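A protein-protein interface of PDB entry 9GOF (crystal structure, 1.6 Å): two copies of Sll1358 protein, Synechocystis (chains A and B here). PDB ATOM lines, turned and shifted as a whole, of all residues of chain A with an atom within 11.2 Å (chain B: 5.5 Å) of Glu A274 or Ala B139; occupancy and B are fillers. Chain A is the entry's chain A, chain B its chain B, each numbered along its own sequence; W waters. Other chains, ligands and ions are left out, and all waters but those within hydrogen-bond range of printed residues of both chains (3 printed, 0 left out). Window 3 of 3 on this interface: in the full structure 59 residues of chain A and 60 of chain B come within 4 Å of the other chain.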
ATOM      1  N   SER A  10      26.240   9.391  25.446  1.00  0.00           N
ATOM      2  CA  SER A  10      27.314  10.358  25.262  1.00  0.00           C
ATOM      3  C   SER A  10      28.405  10.245  26.314  1.00  0.00           C
ATOM      4  O   SER A  10      29.477  10.832  26.130  1.00  0.00           O
ATOM      5  CB  SER A  10      26.761  11.784  25.305  1.00  0.00           C
ATOM      6  OG  SER A  10      26.276  12.059  26.613  1.00  0.00           O
ATOM      7  N   ASN A  11      28.144   9.542  27.417  1.00  0.00           N
ATOM      8  CA  ASN A  11      29.033   9.538  28.582  1.00  0.00           C
ATOM      9  C   ASN A  11      29.238  10.942  29.140  1.00  0.00           C
ATOM     10  O   ASN A  11      30.313  11.269  29.658  1.00  0.00           O
ATOM     11  CB  ASN A  11      30.373   8.884  28.245  1.00  0.00           C
ATOM     12  CG  ASN A  11      30.242   7.398  28.043  1.00  0.00           C
ATOM     13  OD1 ASN A  11      29.605   6.713  28.842  1.00  0.00           O
ATOM     14  ND2 ASN A  11      30.804   6.894  26.959  1.00  0.00           N
ATOM     15  N   VAL A  12      28.197  11.774  29.040  1.00  0.00           N
ATOM     16  CA  VAL A  12      28.256  13.119  29.592  1.00  0.00           C
ATOM     17  C   VAL A  12      28.621  13.058  31.069  1.00  0.00           C
ATOM     18  O   VAL A  12      28.184  12.165  31.807  1.00  0.00           O
ATOM     19  CB  VAL A  12      26.914  13.845  29.386  1.00  0.00           C
ATOM     20  CG1 VAL A  12      25.777  13.097  30.083  1.00  0.00           C
ATOM     21  CG2 VAL A  12      27.003  15.281  29.870  1.00  0.00           C
ATOM     22  N   VAL A  13      29.452  14.000  31.500  1.00  0.00           N
ATOM     23  CA  VAL A  13      29.675  14.202  32.928  1.00  0.00           C
ATOM     24  C   VAL A  13      28.455  14.938  33.470  1.00  0.00           C
ATOM     25  O   VAL A  13      28.269  16.130  33.207  1.00  0.00           O
ATOM     26  CB  VAL A  13      30.962  14.983  33.196  1.00  0.00           C
ATOM     27  CG1 VAL A  13      31.164  15.155  34.700  1.00  0.00           C
ATOM     28  CG2 VAL A  13      32.151  14.267  32.570  1.00  0.00           C
ATOM     29  N   GLY A  15      25.978  17.156  35.237  1.00  0.00           N
ATOM     30  CA  GLY A  15      26.139  18.389  35.978  1.00  0.00           C
ATOM     31  C   GLY A  15      27.280  19.279  35.537  1.00  0.00           C
ATOM     32  O   GLY A  15      27.370  20.420  36.011  1.00  0.00           O
ATOM     33  N   LYS A  16      28.164  18.808  34.656  1.00  0.00           N
ATOM     34  CA  LYS A  16      29.308  19.614  34.255  1.00  0.00           C
ATOM     35  C   LYS A  16      28.839  20.862  33.515  1.00  0.00           C
ATOM     36  O   LYS A  16      28.012  20.775  32.602  1.00  0.00           O
ATOM     37  CB  LYS A  16      30.249  18.802  33.366  1.00  0.00           C
ATOM     38  CG  LYS A  16      31.434  19.603  32.849  1.00  0.00           C
ATOM     39  CD  LYS A  16      32.491  18.695  32.238  1.00  0.00           C
ATOM     40  CE  LYS A  16      33.674  19.506  31.738  1.00  0.00           C
ATOM     41  NZ  LYS A  16      33.963  19.190  30.311  1.00  0.00           N
ATOM     42  N   ASP A  17      29.364  22.022  33.919  1.00  0.00           N
ATOM     43  CA  ASP A  17      29.100  23.310  33.281  1.00  0.00           C
ATOM     44  C   ASP A  17      27.653  23.762  33.425  1.00  0.00           C
ATOM     45  O   ASP A  17      27.183  24.576  32.628  1.00  0.00           O
ATOM     46  CB  ASP A  17      29.493  23.297  31.795  1.00  0.00           C
ATOM     47  CG  ASP A  17      30.982  23.121  31.592  1.00  0.00           C
ATOM     48  OD1 ASP A  17      31.750  23.585  32.462  1.00  0.00           O
ATOM     49  OD2 ASP A  17      31.381  22.520  30.570  1.00  0.00           O
ATOM     50  N   LEU A  18      26.946  23.278  34.443  1.00  0.00           N
ATOM     51  CA  LEU A  18      25.555  23.636  34.670  1.00  0.00           C
ATOM     52  C   LEU A  18      25.346  24.060  36.114  1.00  0.00           C
ATOM     53  O   LEU A  18      26.064  23.599  37.010  1.00  0.00           O
ATOM     54  CB  LEU A  18      24.635  22.448  34.363  1.00  0.00           C
ATOM     55  CG  LEU A  18      24.544  22.085  32.882  1.00  0.00           C
ATOM     56  CD1 LEU A  18      23.694  20.842  32.702  1.00  0.00           C
ATOM     57  CD2 LEU A  18      23.980  23.260  32.094  1.00  0.00           C
ATOM     58  N   PRO A  19      24.365  24.925  36.373  1.00  0.00           N
ATOM     59  CA  PRO A  19      23.956  25.185  37.757  1.00  0.00           C
ATOM     60  C   PRO A  19      23.251  23.973  38.343  1.00  0.00           C
ATOM     61  O   PRO A  19      22.792  23.080  37.630  1.00  0.00           O
ATOM     62  CB  PRO A  19      22.982  26.360  37.625  1.00  0.00           C
ATOM     63  CG  PRO A  19      22.369  26.145  36.242  1.00  0.00           C
ATOM     64  CD  PRO A  19      23.504  25.624  35.396  1.00  0.00           C
ATOM     65  N   PHE A  21      20.169  22.037  39.607  1.00  0.00           N
ATOM     66  CA  PHE A  21      18.728  22.081  39.358  1.00  0.00           C
ATOM     67  C   PHE A  21      17.929  21.533  40.528  1.00  0.00           C
ATOM     68  O   PHE A  21      16.698  21.441  40.440  1.00  0.00           O
ATOM     69  CB  PHE A  21      18.360  21.311  38.085  1.00  0.00           C
ATOM     70  CG  PHE A  21      19.022  21.841  36.850  1.00  0.00           C
ATOM     71  CD1 PHE A  21      18.660  23.070  36.318  1.00  0.00           C
ATOM     72  CD2 PHE A  21      20.031  21.110  36.234  1.00  0.00           C
ATOM     73  CE1 PHE A  21      19.285  23.558  35.182  1.00  0.00           C
ATOM     74  CE2 PHE A  21      20.651  21.587  35.095  1.00  0.00           C
ATOM     75  CZ  PHE A  21      20.278  22.814  34.572  1.00  0.00           C
ATOM     76  N   VAL A 270      17.681  16.619  33.716  1.00  0.00           N
ATOM     77  CA  VAL A 270      17.507  17.918  33.071  1.00  0.00           C
ATOM     78  C   VAL A 270      18.517  18.022  31.936  1.00  0.00           C
ATOM     79  O   VAL A 270      19.721  17.867  32.162  1.00  0.00           O
ATOM     80  CB  VAL A 270      17.707  19.079  34.063  1.00  0.00           C
ATOM     81  CG1 VAL A 270      17.598  20.417  33.331  1.00  0.00           C
ATOM     82  CG2 VAL A 270      16.665  19.014  35.175  1.00  0.00           C
ATOM     83  N   PHE A 271      18.025  18.297  30.729  1.00  0.00           N
ATOM     84  CA  PHE A 271      18.839  18.451  29.527  1.00  0.00           C
ATOM     85  C   PHE A 271      18.846  19.924  29.124  1.00  0.00           C
ATOM     86  O   PHE A 271      17.783  20.522  28.917  1.00  0.00           O
ATOM     87  CB  PHE A 271      18.293  17.577  28.396  1.00  0.00           C
ATOM     88  CG  PHE A 271      18.869  17.909  27.051  1.00  0.00           C
ATOM     89  CD1 PHE A 271      20.229  17.766  26.820  1.00  0.00           C
ATOM     90  CD2 PHE A 271      18.054  18.364  26.025  1.00  0.00           C
ATOM     91  CE1 PHE A 271      20.781  18.084  25.589  1.00  0.00           C
ATOM     92  CE2 PHE A 271      18.599  18.677  24.784  1.00  0.00           C
ATOM     93  CZ  PHE A 271      19.961  18.535  24.574  1.00  0.00           C
ATOM     94  N   ALA A 272      20.041  20.512  29.018  1.00  0.00           N
ATOM     95  CA  ALA A 272      20.175  21.960  28.926  1.00  0.00           C
ATOM     96  C   ALA A 272      20.711  22.444  27.585  1.00  0.00           C
ATOM     97  O   ALA A 272      21.067  23.623  27.475  1.00  0.00           O
ATOM     98  CB  ALA A 272      21.080  22.474  30.053  1.00  0.00           C
ATOM     99  N   SER A 273      20.745  21.575  26.562  1.00  0.00           N
ATOM    100  CA  SER A 273      21.335  21.822  25.240  1.00  0.00           C
ATOM    101  C   SER A 273      22.862  21.865  25.310  1.00  0.00           C
ATOM    102  O   SER A 273      23.448  21.726  26.392  1.00  0.00           O
ATOM    103  CB  SER A 273      20.779  23.109  24.595  1.00  0.00           C
ATOM    104  OG  SER A 273      21.457  24.285  25.032  1.00  0.00           O
ATOM    105  N   GLU A 274      23.510  22.007  24.150  1.00  0.00           N
ATOM    106  CA  GLU A 274      24.971  22.115  24.060  1.00  0.00           C
ATOM    107  C   GLU A 274      25.671  20.932  24.724  1.00  0.00           C
ATOM    108  O   GLU A 274      26.749  21.081  25.301  1.00  0.00           O
ATOM    109  CB  GLU A 274      25.458  23.439  24.654  1.00  0.00           C
ATOM    110  CG  GLU A 274      24.767  24.654  24.025  1.00  0.00           C
ATOM    111  CD  GLU A 274      25.187  25.975  24.642  1.00  0.00           C
ATOM    112  OE1 GLU A 274      25.561  25.999  25.835  1.00  0.00           O
ATOM    113  OE2 GLU A 274      25.129  26.999  23.931  1.00  0.00           O
ATOM    114  N   GLY A 275      25.058  19.754  24.646  1.00  0.00           N
ATOM    115  CA  GLY A 275      25.668  18.551  25.200  1.00  0.00           C
ATOM    116  C   GLY A 275      25.835  18.569  26.706  1.00  0.00           C
ATOM    117  O   GLY A 275      26.740  17.905  27.229  1.00  0.00           O
ATOM    118  N   LYS A 276      24.987  19.313  27.420  1.00  0.00           N
ATOM    119  CA  LYS A 276      25.053  19.415  28.874  1.00  0.00           C
ATOM    120  C   LYS A 276      23.769  18.879  29.495  1.00  0.00           C
ATOM    121  O   LYS A 276      22.667  19.174  29.019  1.00  0.00           O
ATOM    122  CB  LYS A 276      25.281  20.867  29.314  1.00  0.00           C
ATOM    123  CG  LYS A 276      26.571  21.474  28.764  1.00  0.00           C
ATOM    124  CD  LYS A 276      26.634  22.991  28.990  1.00  0.00           C
ATOM    125  CE  LYS A 276      27.616  23.642  28.013  1.00  0.00           C
ATOM    126  NZ  LYS A 276      27.367  25.107  27.844  1.00  0.00           N
ATOM    127  N   ALA A 277      23.912  18.105  30.573  1.00  0.00           N
ATOM    128  CA  ALA A 277      22.749  17.551  31.248  1.00  0.00           C
ATOM    129  C   ALA A 277      23.126  17.153  32.665  1.00  0.00           C
ATOM    130  O   ALA A 277      24.305  17.010  32.994  1.00  0.00           O
ATOM    131  CB  ALA A 277      22.185  16.345  30.491  1.00  0.00           C
ATOM    132  N   SER A 278      22.093  16.958  33.492  1.00  0.00           N
ATOM    133  CA  SER A 278      22.251  16.600  34.896  1.00  0.00           C
ATOM    134  C   SER A 278      21.258  15.507  35.263  1.00  0.00           C
ATOM    135  O   SER A 278      20.214  15.343  34.630  1.00  0.00           O
ATOM    136  CB  SER A 278      22.026  17.811  35.821  1.00  0.00           C
ATOM    137  OG  SER A 278      22.876  18.884  35.470  1.00  0.00           O
ATOM    138  N   LYS A 292      12.524  27.099  31.686  1.00  0.00           N
ATOM    139  CA  LYS A 292      11.728  27.075  30.461  1.00  0.00           C
ATOM    140  C   LYS A 292      12.497  26.483  29.290  1.00  0.00           C
ATOM    141  O   LYS A 292      13.604  26.921  28.976  1.00  0.00           O
ATOM    142  CB  LYS A 292      11.291  28.498  30.103  1.00  0.00           C
ATOM    143  CG  LYS A 292      10.297  28.521  28.938  1.00  0.00           C
ATOM    144  CD  LYS A 292       9.861  29.942  28.564  1.00  0.00           C
ATOM    145  CE  LYS A 292      11.022  30.850  28.236  1.00  0.00           C
ATOM    146  NZ  LYS A 292      10.519  32.225  27.944  1.00  0.00           N
ATOM    147  N   GLY A 293      11.891  25.494  28.634  1.00  0.00           N
ATOM    148  CA  GLY A 293      12.467  24.912  27.445  1.00  0.00           C
ATOM    149  C   GLY A 293      13.425  23.763  27.682  1.00  0.00           C
ATOM    150  O   GLY A 293      13.738  23.038  26.731  1.00  0.00           O
ATOM    151  N   TYR A 294      13.910  23.562  28.906  1.00  0.00           N
ATOM    152  CA  TYR A 294      14.861  22.477  29.116  1.00  0.00           C
ATOM    153  C   TYR A 294      14.128  21.143  29.085  1.00  0.00           C
ATOM    154  O   TYR A 294      13.025  21.013  29.618  1.00  0.00           O
ATOM    155  CB  TYR A 294      15.589  22.644  30.455  1.00  0.00           C
ATOM    156  CG  TYR A 294      16.667  23.708  30.495  1.00  0.00           C
ATOM    157  CD1 TYR A 294      16.643  24.811  29.642  1.00  0.00           C
ATOM    158  CD2 TYR A 294      17.709  23.615  31.415  1.00  0.00           C
ATOM    159  CE1 TYR A 294      17.634  25.781  29.703  1.00  0.00           C
ATOM    160  CE2 TYR A 294      18.694  24.573  31.483  1.00  0.00           C
ATOM    161  CZ  TYR A 294      18.658  25.656  30.633  1.00  0.00           C
ATOM    162  OH  TYR A 294      19.654  26.611  30.720  1.00  0.00           O
ATOM    163  N   GLY A 295      14.735  20.144  28.446  1.00  0.00           N
ATOM    164  CA  GLY A 295      14.140  18.817  28.463  1.00  0.00           C
ATOM    165  C   GLY A 295      14.270  18.180  29.839  1.00  0.00           C
ATOM    166  O   GLY A 295      15.257  18.377  30.549  1.00  0.00           O
ATOM    167  N   TRP B  69      14.271  22.258  19.016  1.00  0.00           N
ATOM    168  CA  TRP B  69      13.405  23.347  19.455  1.00  0.00           C
ATOM    169  C   TRP B  69      14.258  24.424  20.101  1.00  0.00           C
ATOM    170  O   TRP B  69      15.439  24.215  20.389  1.00  0.00           O
ATOM    171  CB  TRP B  69      12.305  22.846  20.414  1.00  0.00           C
ATOM    172  CG  TRP B  69      12.748  22.550  21.834  1.00  0.00           C
ATOM    173  CD1 TRP B  69      12.706  23.412  22.910  1.00  0.00           C
ATOM    174  CD2 TRP B  69      13.261  21.304  22.342  1.00  0.00           C
ATOM    175  NE1 TRP B  69      13.174  22.779  24.042  1.00  0.00           N
ATOM    176  CE2 TRP B  69      13.520  21.489  23.722  1.00  0.00           C
ATOM    177  CE3 TRP B  69      13.546  20.057  21.759  1.00  0.00           C
ATOM    178  CZ2 TRP B  69      14.041  20.471  24.535  1.00  0.00           C
ATOM    179  CZ3 TRP B  69      14.062  19.044  22.569  1.00  0.00           C
ATOM    180  CH2 TRP B  69      14.305  19.261  23.940  1.00  0.00           C
ATOM    181  N   HIS B  70      13.647  25.600  20.318  1.00  0.00           N
ATOM    182  CA  HIS B  70      14.338  26.684  21.015  1.00  0.00           C
ATOM    183  C   HIS B  70      13.260  27.605  21.588  1.00  0.00           C
ATOM    184  O   HIS B  70      12.659  28.394  20.850  1.00  0.00           O
ATOM    185  CB  HIS B  70      15.290  27.438  20.095  1.00  0.00           C
ATOM    186  CG  HIS B  70      14.921  27.379  18.642  1.00  0.00           C
ATOM    187  ND1 HIS B  70      13.882  28.114  18.107  1.00  0.00           N
ATOM    188  CD2 HIS B  70      15.472  26.696  17.609  1.00  0.00           C
ATOM    189  CE1 HIS B  70      13.800  27.871  16.807  1.00  0.00           C
ATOM    190  NE2 HIS B  70      14.750  27.010  16.483  1.00  0.00           N
ATOM    191  N   ASN B  72      13.576  30.095  23.479  1.00  0.00           N
ATOM    192  CA  ASN B  72      14.018  31.475  23.586  1.00  0.00           C
ATOM    193  C   ASN B  72      13.740  32.319  22.346  1.00  0.00           C
ATOM    194  O   ASN B  72      13.929  33.535  22.411  1.00  0.00           O
ATOM    195  CB  ASN B  72      15.521  31.523  23.922  1.00  0.00           C
ATOM    196  CG  ASN B  72      16.404  31.026  22.769  1.00  0.00           C
ATOM    197  OD1 ASN B  72      16.150  29.966  22.199  1.00  0.00           O
ATOM    198  ND2 ASN B  72      17.411  31.809  22.398  1.00  0.00           N
ATOM    199  N   SER B 136      21.597  31.690  18.839  1.00  0.00           N
ATOM    200  CA  SER B 136      22.678  31.017  18.126  1.00  0.00           C
ATOM    201  C   SER B 136      22.236  29.614  17.726  1.00  0.00           C
ATOM    202  O   SER B 136      21.620  28.899  18.524  1.00  0.00           O
ATOM    203  CB  SER B 136      23.956  30.934  18.988  1.00  0.00           C
ATOM    204  OG  SER B 136      24.859  29.967  18.444  1.00  0.00           O
ATOM    205  N   GLU B 137      22.561  29.219  16.489  1.00  0.00           N
ATOM    206  CA  GLU B 137      22.257  27.863  16.033  1.00  0.00           C
ATOM    207  C   GLU B 137      23.017  26.809  16.828  1.00  0.00           C
ATOM    208  O   GLU B 137      22.643  25.630  16.787  1.00  0.00           O
ATOM    209  CB  GLU B 137      22.587  27.699  14.541  1.00  0.00           C
ATOM    210  CG  GLU B 137      21.493  28.182  13.579  1.00  0.00           C
ATOM    211  CD  GLU B 137      20.280  27.263  13.505  1.00  0.00           C
ATOM    212  OE1 GLU B 137      20.437  26.041  13.684  1.00  0.00           O
ATOM    213  OE2 GLU B 137      19.162  27.760  13.237  1.00  0.00           O
ATOM    214  N   GLY B 138      24.072  27.197  17.542  1.00  0.00           N
ATOM    215  CA  GLY B 138      24.792  26.253  18.385  1.00  0.00           C
ATOM    216  C   GLY B 138      24.127  25.986  19.718  1.00  0.00           C
ATOM    217  O   GLY B 138      24.555  25.088  20.454  1.00  0.00           O
ATOM    218  N   ALA B 139      23.064  26.727  20.019  1.00  0.00           N
ATOM    219  CA  ALA B 139      22.390  26.637  21.308  1.00  0.00           C
ATOM    220  C   ALA B 139      20.934  26.204  21.168  1.00  0.00           C
ATOM    221  O   ALA B 139      20.091  26.572  21.989  1.00  0.00           O
ATOM    222  CB  ALA B 139      22.479  27.971  22.048  1.00  0.00           C
ATOM    223  N   THR B 140      20.611  25.434  20.135  1.00  0.00           N
ATOM    224  CA  THR B 140      19.270  24.877  20.040  1.00  0.00           C
ATOM    225  C   THR B 140      19.220  23.547  20.784  1.00  0.00           C
ATOM    226  O   THR B 140      20.247  22.941  21.092  1.00  0.00           O
ATOM    227  CB  THR B 140      18.826  24.692  18.583  1.00  0.00           C
ATOM    228  OG1 THR B 140      19.451  23.526  18.017  1.00  0.00           O
ATOM    229  CG2 THR B 140      19.178  25.933  17.752  1.00  0.00           C
ATOM    230  N   PHE B 141      18.001  23.107  21.082  1.00  0.00           N
ATOM    231  CA  PHE B 141      17.771  21.869  21.818  1.00  0.00           C
ATOM    232  C   PHE B 141      17.521  20.754  20.812  1.00  0.00           C
ATOM    233  O   PHE B 141      16.460  20.700  20.185  1.00  0.00           O
ATOM    234  CB  PHE B 141      16.605  22.048  22.789  1.00  0.00           C
ATOM    235  CG  PHE B 141      16.969  22.853  24.007  1.00  0.00           C
ATOM    236  CD1 PHE B 141      17.141  24.225  23.917  1.00  0.00           C
ATOM    237  CD2 PHE B 141      17.189  22.230  25.237  1.00  0.00           C
ATOM    238  CE1 PHE B 141      17.506  24.971  25.040  1.00  0.00           C
ATOM    239  CE2 PHE B 141      17.557  22.966  26.363  1.00  0.00           C
ATOM    240  CZ  PHE B 141      17.707  24.339  26.262  1.00  0.00           C
ATOM    241  N   ASP B 145      20.925  15.118  20.649  1.00  0.00           N
ATOM    242  CA  ASP B 145      21.626  15.543  21.862  1.00  0.00           C
ATOM    243  C   ASP B 145      20.845  15.122  23.106  1.00  0.00           C
ATOM    244  O   ASP B 145      21.408  14.570  24.056  1.00  0.00           O
ATOM    245  CB  ASP B 145      21.830  17.068  21.807  1.00  0.00           C
ATOM    246  CG  ASP B 145      22.957  17.571  22.710  1.00  0.00           C
ATOM    247  OD1 ASP B 145      23.802  16.766  23.167  1.00  0.00           O
ATOM    248  OD2 ASP B 145      23.001  18.801  22.938  1.00  0.00           O
ATOM    249  N   GLN B 173      24.901  15.425  19.458  1.00  0.00           N
ATOM    250  CA  GLN B 173      24.025  16.245  18.620  1.00  0.00           C
ATOM    251  C   GLN B 173      24.380  16.072  17.141  1.00  0.00           C
ATOM    252  O   GLN B 173      25.530  16.274  16.736  1.00  0.00           O
ATOM    253  CB  GLN B 173      24.142  17.712  19.041  1.00  0.00           C
ATOM    254  CG  GLN B 173      23.563  18.707  18.029  1.00  0.00           C
ATOM    255  CD  GLN B 173      23.348  20.111  18.594  1.00  0.00           C
ATOM    256  OE1 GLN B 173      22.608  20.903  18.014  1.00  0.00           O
ATOM    257  NE2 GLN B 173      23.978  20.415  19.731  1.00  0.00           N
HETATM  258  O   HOH W   1      23.025  22.874  21.334  1.00  0.00           O
HETATM  259  O   HOH W   2      20.483  26.939  24.863  1.00  0.00           O
HETATM  260  O   HOH W   3      14.358  25.761  24.685  1.00  0.00           O
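The side-chain carboxylate (OD2) of Asp B145 sits at hydrogen-bond distance from the backbone NH (N) of Glu A274, at 3.5 Å.
The side-chain carboxylate (OD2) of Asp B145 is in hydrogen-bond range of the backbone NH (N) of Gly A275 (2.8 Å).
The indole nitrogen (NE1) of Trp B69 is in hydrogen-bond range of the backbone carbonyl oxygen (O) of Gly A293, at 2.8 Å.
The backbone NH of Phe A271 sits at hydrogen-bond distance from the backbone carbonyl oxygen of Gly A295, 2.8 Å away.
OE1 of Glu A274 is in salt-bridge range of NZ of Lys A276 (2.8 Å).
The backbone carbonyl oxygen of Trp B69 is in hydrogen-bond range of the backbone NH of Phe B141 (2.9 Å).
The side-chain hydroxyl (OG) of Ser B136 is in hydrogen-bond range of the backbone NH (N) of Gly B138.
Among the printed residues, merely in contact across the chains: Phe A271 with Phe B141 (3.5 Å), Phe A271 with Asp B145 (3.5 Å), Ala A272 with Phe B141 (3.4 Å), Ser A273 with Thr B140 (3.5 Å), Ser A273 with Phe B141 (3.5 Å), Ser A273 with Asp B145 (3.9 Å), Glu A274 with Gly B138 (3.6 Å), Glu A274 with Ala B139 (3.4 Å), Gly A293 with Phe B141 (3.8 Å), Tyr A294 with Phe B141 (3.6 Å) and Gly A295 with Trp B69 (3.99 Å).
Of the printed residues of chain B, Ser A273 touches Thr B140, Phe B141 and Asp B145.
Of chain B, only Gly B138, Ala B139 and Asp B145 come within 4 Å of Glu A274.
Printed residues of chain B within 4 Å of Gly A293: Trp B69 (2.8 Å) and Phe B141 (3.8 Å).
Of the printed residues of chain B, Tyr A294 touches Phe B141.
Of the printed residues of chain B, Gly A295 touches Trp B69.
No residue of chain A comes within 4 Å of Ser B136.
Gly B138 touches just one residue of chain A: Glu A274.
Thr B140 touches just one residue of chain A: Ser A273.
Of chain A, only Phe A271 (3.5 Å), Ala A272 (3.4 Å), Ser A273 (3.5 Å), Gly A293 (3.8 Å) and Tyr A294 (3.6 Å) come within 4 Å of Phe B141.
The nearest residue of chain B that does not touch Glu A274 is Thr B140 (4.6 Å).
The nearest residue of chain A that does not touch Ala B139 is Ser A273 (4.04 Å).
Hydrophobic or aromatic side chains of chain A within 4 Å of the printed part of chain B: Phe A271 and Tyr A294.
Hydrophobic or aromatic side chains of chain B within 4 Å of the printed part of chain A: Trp B69, Ala B139 and Phe B141.
Among the printed residues, 14 pairs touch across the chains.
Among the printed residues, no Asp or Glu carboxylate lies within 4 Å of a Lys or Arg side-chain nitrogen of the other chain.
No position is printed for both chains.
Of the 14 pairs that touch across the chains among the printed residues, none has its exchanged pair printed and touching as well.
Water W1 lies within hydrogen-bond range of the backbone carbonyl oxygen of Thr B140 (2.8 Å), the backbone carbonyl oxygen of Gly B138 (2.8 Å), the backbone NH of Glu A274 (3.0 Å) and the side-chain amide nitrogen of Gln B173 (3.1 Å).
Water W2 lies within hydrogen-bond range of the side-chain hydroxyl (OG) of Ser A273 (2.8 Å) and the backbone carbonyl oxygen (O) of Ala B139 (2.9 Å).
Water W3 bridges NE1 of Trp B69 (3.3 Å) and O of Gly A293 (3.5 Å).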
